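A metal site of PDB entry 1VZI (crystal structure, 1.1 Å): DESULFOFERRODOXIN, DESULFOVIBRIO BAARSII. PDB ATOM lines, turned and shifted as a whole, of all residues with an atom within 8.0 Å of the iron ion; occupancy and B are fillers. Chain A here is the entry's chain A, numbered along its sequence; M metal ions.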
ATOM      1  N   VAL A  42      14.743 -20.532 -24.003  1.00  0.00           N
ATOM      2  CA  VAL A  42      13.472 -20.975 -23.433  1.00  0.00           C
ATOM      3  C   VAL A  42      12.630 -19.801 -22.953  1.00  0.00           C
ATOM      4  O   VAL A  42      13.138 -18.774 -22.504  1.00  0.00           O
ATOM      5  CB  VAL A  42      13.805 -21.908 -22.269  1.00  0.00           C
ATOM      6  CG1 VAL A  42      12.607 -22.160 -21.370  1.00  0.00           C
ATOM      7  CG2 VAL A  42      14.407 -23.250 -22.766  1.00  0.00           C
ATOM      8  N   ALA A  44      10.987 -18.240 -20.346  1.00  0.00           N
ATOM      9  CA  ALA A  44      11.024 -18.333 -18.881  1.00  0.00           C
ATOM     10  C   ALA A  44      11.398 -16.964 -18.347  1.00  0.00           C
ATOM     11  O   ALA A  44      11.869 -16.095 -19.089  1.00  0.00           O
ATOM     12  CB  ALA A  44      11.990 -19.429 -18.461  1.00  0.00           C
ATOM     13  N   ALA A  45      11.199 -16.771 -17.034  1.00  0.00           N
ATOM     14  CA  ALA A  45      11.514 -15.451 -16.467  1.00  0.00           C
ATOM     15  C   ALA A  45      12.999 -15.157 -16.503  1.00  0.00           C
ATOM     16  O   ALA A  45      13.791 -15.806 -15.806  1.00  0.00           O
ATOM     17  CB  ALA A  45      11.014 -15.328 -15.016  1.00  0.00           C
ATOM     18  N   LYS A  48      14.818 -14.445 -13.173  1.00  0.00           N
ATOM     19  CA  LYS A  48      15.194 -15.553 -12.311  1.00  0.00           C
ATOM     20  C   LYS A  48      16.217 -16.489 -12.960  1.00  0.00           C
ATOM     21  O   LYS A  48      16.738 -17.375 -12.256  1.00  0.00           O
ATOM     22  CB  LYS A  48      13.953 -16.401 -11.914  1.00  0.00           C
ATOM     23  CG  LYS A  48      13.022 -15.547 -11.003  1.00  0.00           C
ATOM     24  CD  LYS A  48      12.083 -16.467 -10.219  1.00  0.00           C
ATOM     25  CE  LYS A  48      10.998 -15.567  -9.601  1.00  0.00           C
ATOM     26  NZ  LYS A  48      10.076 -16.383  -8.800  1.00  0.00           N
ATOM     27  N   HIS A  49      16.464 -16.313 -14.256  1.00  0.00           N
ATOM     28  CA  HIS A  49      17.343 -17.266 -14.944  1.00  0.00           C
ATOM     29  C   HIS A  49      18.617 -16.679 -15.517  1.00  0.00           C
ATOM     30  O   HIS A  49      19.607 -17.412 -15.660  1.00  0.00           O
ATOM     31  CB  HIS A  49      16.584 -17.966 -16.101  1.00  0.00           C
ATOM     32  CG  HIS A  49      15.554 -18.903 -15.571  1.00  0.00           C
ATOM     33  ND1 HIS A  49      14.239 -18.467 -15.357  1.00  0.00           N
ATOM     34  CD2 HIS A  49      15.586 -20.173 -15.157  1.00  0.00           C
ATOM     35  CE1 HIS A  49      13.506 -19.493 -14.847  1.00  0.00           C
ATOM     36  NE2 HIS A  49      14.309 -20.547 -14.717  1.00  0.00           N
ATOM     37  N   VAL A  64      21.780 -16.501  -9.488  1.00  0.00           N
ATOM     38  CA  VAL A  64      20.741 -16.839 -10.486  1.00  0.00           C
ATOM     39  C   VAL A  64      19.365 -16.511  -9.887  1.00  0.00           C
ATOM     40  O   VAL A  64      18.902 -17.261  -9.032  1.00  0.00           O
ATOM     41  CB  VAL A  64      20.842 -18.326 -10.860  1.00  0.00           C
ATOM     42  CG1 VAL A  64      19.788 -18.670 -11.874  1.00  0.00           C
ATOM     43  CG2 VAL A  64      22.276 -18.600 -11.387  1.00  0.00           C
ATOM     44  N   HIS A  69      16.281 -17.539  -7.899  1.00  0.00           N
ATOM     45  CA  HIS A  69      15.462 -18.608  -8.470  1.00  0.00           C
ATOM     46  C   HIS A  69      15.100 -19.640  -7.422  1.00  0.00           C
ATOM     47  O   HIS A  69      15.866 -19.875  -6.460  1.00  0.00           O
ATOM     48  CB  HIS A  69      16.339 -19.247  -9.594  1.00  0.00           C
ATOM     49  CG  HIS A  69      15.657 -20.313 -10.365  1.00  0.00           C
ATOM     50  ND1 HIS A  69      15.480 -21.609  -9.927  1.00  0.00           N
ATOM     51  CD2 HIS A  69      15.088 -20.242 -11.603  1.00  0.00           C
ATOM     52  CE1 HIS A  69      14.802 -22.318 -10.855  1.00  0.00           C
ATOM     53  NE2 HIS A  69      14.563 -21.513 -11.880  1.00  0.00           N
ATOM     54  N   PRO A  70      13.947 -20.318  -7.518  1.00  0.00           N
ATOM     55  CA  PRO A  70      13.641 -21.387  -6.557  1.00  0.00           C
ATOM     56  C   PRO A  70      14.708 -22.477  -6.504  1.00  0.00           C
ATOM     57  O   PRO A  70      15.463 -22.729  -7.477  1.00  0.00           O
ATOM     58  CB  PRO A  70      12.362 -22.011  -7.153  1.00  0.00           C
ATOM     59  CG  PRO A  70      11.745 -20.902  -7.911  1.00  0.00           C
ATOM     60  CD  PRO A  70      12.866 -20.087  -8.499  1.00  0.00           C
ATOM     61  N   LYS A  74      11.767 -30.284  -7.289  1.00  0.00           N
ATOM     62  CA  LYS A  74      11.505 -30.551  -8.707  1.00  0.00           C
ATOM     63  C   LYS A  74      11.702 -29.273  -9.548  1.00  0.00           C
ATOM     64  O   LYS A  74      11.305 -29.205 -10.754  1.00  0.00           O
ATOM     65  CB  LYS A  74      10.121 -31.205  -8.912  1.00  0.00           C
ATOM     66  CG  LYS A  74       9.958 -32.540  -8.182  1.00  0.00           C
ATOM     67  CD  LYS A  74       8.743 -33.326  -8.669  1.00  0.00           C
ATOM     68  CE  LYS A  74       8.656 -34.591  -7.789  1.00  0.00           C
ATOM     69  NZ  LYS A  74       7.574 -35.529  -8.219  1.00  0.00           N
ATOM     70  N   HIS A  75      12.280 -28.242  -8.994  1.00  0.00           N
ATOM     71  CA  HIS A  75      12.577 -27.034  -9.733  1.00  0.00           C
ATOM     72  C   HIS A  75      13.746 -26.308  -9.091  1.00  0.00           C
ATOM     73  O   HIS A  75      13.569 -25.601  -8.081  1.00  0.00           O
ATOM     74  CB  HIS A  75      11.346 -26.091  -9.787  1.00  0.00           C
ATOM     75  CG  HIS A  75      11.626 -24.937 -10.715  1.00  0.00           C
ATOM     76  ND1 HIS A  75      10.969 -23.755 -10.587  1.00  0.00           N
ATOM     77  CD2 HIS A  75      12.500 -24.775 -11.739  1.00  0.00           C
ATOM     78  CE1 HIS A  75      11.393 -22.887 -11.503  1.00  0.00           C
ATOM     79  NE2 HIS A  75      12.339 -23.504 -12.229  1.00  0.00           N
ATOM     80  N   TYR A  76      14.946 -26.516  -9.678  1.00  0.00           N
ATOM     81  CA  TYR A  76      16.121 -25.939  -9.046  1.00  0.00           C
ATOM     82  C   TYR A  76      17.190 -25.723 -10.134  1.00  0.00           C
ATOM     83  O   TYR A  76      17.171 -26.316 -11.199  1.00  0.00           O
ATOM     84  CB  TYR A  76      16.650 -26.746  -7.848  1.00  0.00           C
ATOM     85  CG  TYR A  76      17.233 -28.125  -8.179  1.00  0.00           C
ATOM     86  CD1 TYR A  76      16.382 -29.152  -8.555  1.00  0.00           C
ATOM     87  CD2 TYR A  76      18.609 -28.306  -8.150  1.00  0.00           C
ATOM     88  CE1 TYR A  76      16.913 -30.402  -8.871  1.00  0.00           C
ATOM     89  CE2 TYR A  76      19.155 -29.583  -8.458  1.00  0.00           C
ATOM     90  CZ  TYR A  76      18.288 -30.607  -8.809  1.00  0.00           C
ATOM     91  OH  TYR A  76      18.814 -31.838  -9.115  1.00  0.00           O
ATOM     92  N   ILE A  77      18.139 -24.850  -9.773  1.00  0.00           N
ATOM     93  CA  ILE A  77      19.358 -24.658 -10.589  1.00  0.00           C
ATOM     94  C   ILE A  77      20.296 -25.772 -10.275  1.00  0.00           C
ATOM     95  O   ILE A  77      20.787 -25.927  -9.141  1.00  0.00           O
ATOM     96  CB  ILE A  77      19.973 -23.295 -10.264  1.00  0.00           C
ATOM     97  CG1 ILE A  77      18.946 -22.150 -10.428  1.00  0.00           C
ATOM     98  CG2 ILE A  77      21.231 -23.097 -11.092  1.00  0.00           C
ATOM     99  CD1 ILE A  77      18.202 -22.204 -11.771  1.00  0.00           C
ATOM    100  N   GLU A 114      24.151 -21.048 -16.285  1.00  0.00           N
ATOM    101  CA  GLU A 114      23.416 -21.836 -15.271  1.00  0.00           C
ATOM    102  C   GLU A 114      22.444 -22.766 -16.039  1.00  0.00           C
ATOM    103  O   GLU A 114      21.976 -22.385 -17.115  1.00  0.00           O
ATOM    104  CB  GLU A 114      22.688 -20.932 -14.237  1.00  0.00           C
ATOM    105  CG  GLU A 114      21.586 -20.071 -14.858  1.00  0.00           C
ATOM    106  CD  GLU A 114      20.199 -20.702 -14.875  1.00  0.00           C
ATOM    107  OE1 GLU A 114      20.075 -21.871 -14.548  1.00  0.00           O
ATOM    108  OE2 GLU A 114      19.207 -19.979 -15.255  1.00  0.00           O
ATOM    109  N   TYR A 115      22.142 -23.894 -15.410  1.00  0.00           N
ATOM    110  CA  TYR A 115      21.123 -24.777 -15.990  1.00  0.00           C
ATOM    111  C   TYR A 115      20.035 -25.020 -14.957  1.00  0.00           C
ATOM    112  O   TYR A 115      20.305 -25.478 -13.826  1.00  0.00           O
ATOM    113  CB  TYR A 115      21.825 -26.101 -16.404  1.00  0.00           C
ATOM    114  CG  TYR A 115      20.837 -26.986 -17.129  1.00  0.00           C
ATOM    115  CD1 TYR A 115      20.095 -27.958 -16.442  1.00  0.00           C
ATOM    116  CD2 TYR A 115      20.606 -26.839 -18.487  1.00  0.00           C
ATOM    117  CE1 TYR A 115      19.173 -28.764 -17.069  1.00  0.00           C
ATOM    118  CE2 TYR A 115      19.649 -27.649 -19.123  1.00  0.00           C
ATOM    119  CZ  TYR A 115      18.950 -28.603 -18.420  1.00  0.00           C
ATOM    120  OH  TYR A 115      18.035 -29.383 -19.061  1.00  0.00           O
ATOM    121  N   CYS A 116      18.799 -24.761 -15.381  1.00  0.00           N
ATOM    122  CA  CYS A 116      17.590 -25.013 -14.583  1.00  0.00           C
ATOM    123  C   CYS A 116      16.954 -26.313 -15.055  1.00  0.00           C
ATOM    124  O   CYS A 116      16.798 -26.533 -16.268  1.00  0.00           O
ATOM    125  CB  CYS A 116      16.611 -23.802 -14.789  1.00  0.00           C
ATOM    126  SG  CYS A 116      15.004 -24.227 -13.971  1.00  0.00           S
ATOM    127  N   ASN A 117      16.594 -27.218 -14.134  1.00  0.00           N
ATOM    128  CA  ASN A 117      16.078 -28.497 -14.632  1.00  0.00           C
ATOM    129  C   ASN A 117      14.785 -28.312 -15.420  1.00  0.00           C
ATOM    130  O   ASN A 117      14.499 -29.182 -16.255  1.00  0.00           O
ATOM    131  CB  ASN A 117      15.817 -29.457 -13.496  1.00  0.00           C
ATOM    132  CG  ASN A 117      14.640 -29.078 -12.616  1.00  0.00           C
ATOM    133  OD1 ASN A 117      14.540 -27.933 -12.117  1.00  0.00           O
ATOM    134  ND2 ASN A 117      13.686 -29.968 -12.407  1.00  0.00           N
ATOM    135  N   ILE A 118      14.033 -27.241 -15.179  1.00  0.00           N
ATOM    136  CA  ILE A 118      12.813 -27.034 -15.960  1.00  0.00           C
ATOM    137  C   ILE A 118      13.049 -26.084 -17.151  1.00  0.00           C
ATOM    138  O   ILE A 118      12.582 -26.355 -18.265  1.00  0.00           O
ATOM    139  CB  ILE A 118      11.698 -26.456 -15.042  1.00  0.00           C
ATOM    140  CG1 ILE A 118      11.333 -27.491 -13.940  1.00  0.00           C
ATOM    141  CG2 ILE A 118      10.488 -26.068 -15.893  1.00  0.00           C
ATOM    142  CD1 ILE A 118      10.075 -27.120 -13.172  1.00  0.00           C
ATOM    143  N   HIS A 119      13.789 -25.002 -16.892  1.00  0.00           N
ATOM    144  CA  HIS A 119      13.869 -23.899 -17.870  1.00  0.00           C
ATOM    145  C   HIS A 119      15.162 -23.850 -18.655  1.00  0.00           C
ATOM    146  O   HIS A 119      15.368 -22.899 -19.428  1.00  0.00           O
ATOM    147  CB  HIS A 119      13.651 -22.564 -17.164  1.00  0.00           C
ATOM    148  CG  HIS A 119      12.297 -22.523 -16.506  1.00  0.00           C
ATOM    149  ND1 HIS A 119      12.102 -22.439 -15.153  1.00  0.00           N
ATOM    150  CD2 HIS A 119      11.047 -22.590 -17.096  1.00  0.00           C
ATOM    151  CE1 HIS A 119      10.780 -22.442 -14.930  1.00  0.00           C
ATOM    152  NE2 HIS A 119      10.115 -22.513 -16.096  1.00  0.00           N
ATOM    153  N   GLY A 120      15.957 -24.919 -18.532  1.00  0.00           N
ATOM    154  CA  GLY A 120      17.138 -25.033 -19.456  1.00  0.00           C
ATOM    155  C   GLY A 120      18.306 -24.106 -19.157  1.00  0.00           C
ATOM    156  O   GLY A 120      18.590 -23.740 -18.016  1.00  0.00           O
ATOM    157  N   TRP A 122      21.135 -21.005 -19.516  1.00  0.00           N
ATOM    158  CA  TRP A 122      21.167 -19.550 -19.567  1.00  0.00           C
ATOM    159  C   TRP A 122      22.596 -19.041 -19.352  1.00  0.00           C
ATOM    160  O   TRP A 122      23.390 -19.679 -18.636  1.00  0.00           O
ATOM    161  CB  TRP A 122      20.251 -18.916 -18.463  1.00  0.00           C
ATOM    162  CG  TRP A 122      18.816 -19.302 -18.802  1.00  0.00           C
ATOM    163  CD1 TRP A 122      18.144 -20.465 -18.529  1.00  0.00           C
ATOM    164  CD2 TRP A 122      17.878 -18.465 -19.512  1.00  0.00           C
ATOM    165  NE1 TRP A 122      16.866 -20.416 -19.048  1.00  0.00           N
ATOM    166  CE2 TRP A 122      16.669 -19.177 -19.650  1.00  0.00           C
ATOM    167  CE3 TRP A 122      17.976 -17.179 -20.030  1.00  0.00           C
ATOM    168  CZ2 TRP A 122      15.523 -18.684 -20.278  1.00  0.00           C
ATOM    169  CZ3 TRP A 122      16.830 -16.696 -20.667  1.00  0.00           C
ATOM    170  CH2 TRP A 122      15.650 -17.395 -20.805  1.00  0.00           C
HETATM  171 FE    FE M   1      13.628 -22.329 -13.634  1.00  0.00          FE
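N of His 69 is in hydrogen-bond range of O of Val 64 (2.9 Å).
O of His 119 lies within hydrogen-bond range of NE1 of Trp 122 (2.9 Å).
The backbone carbonyl oxygen of His 49 sits close to the side-chain carboxylate of Glu 114 (2.6 Å).
A ring nitrogen (ND1) of His 49 lies within hydrogen-bond range of the backbone carbonyl oxygen (O) of Ala 45.
The side-chain sulfur (SG) of Cys 116 sits close to the backbone NH (N) of Ile 118.
N of Cys 116 is in hydrogen-bond range of OE1 of Glu 114 (3.3 Å).
Five residues have an atom within 4 Å of the iron ion: His 49, His 69, His 75, Cys 116 and His 119.
The nearest printed residue that does not touch the iron ion is Ile 118 (4.8 Å).
The iron ion is bound by a ring nitrogen (NE2) of His 69 (2.1 Å), a ring nitrogen (ND1) of His 119 (2.2 Å), a ring nitrogen (NE2) of His 49 (2.2 Å), a ring nitrogen (NE2) of His 75 (2.2 Å) and the side-chain sulfur of Cys 116 (2.4 Å).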
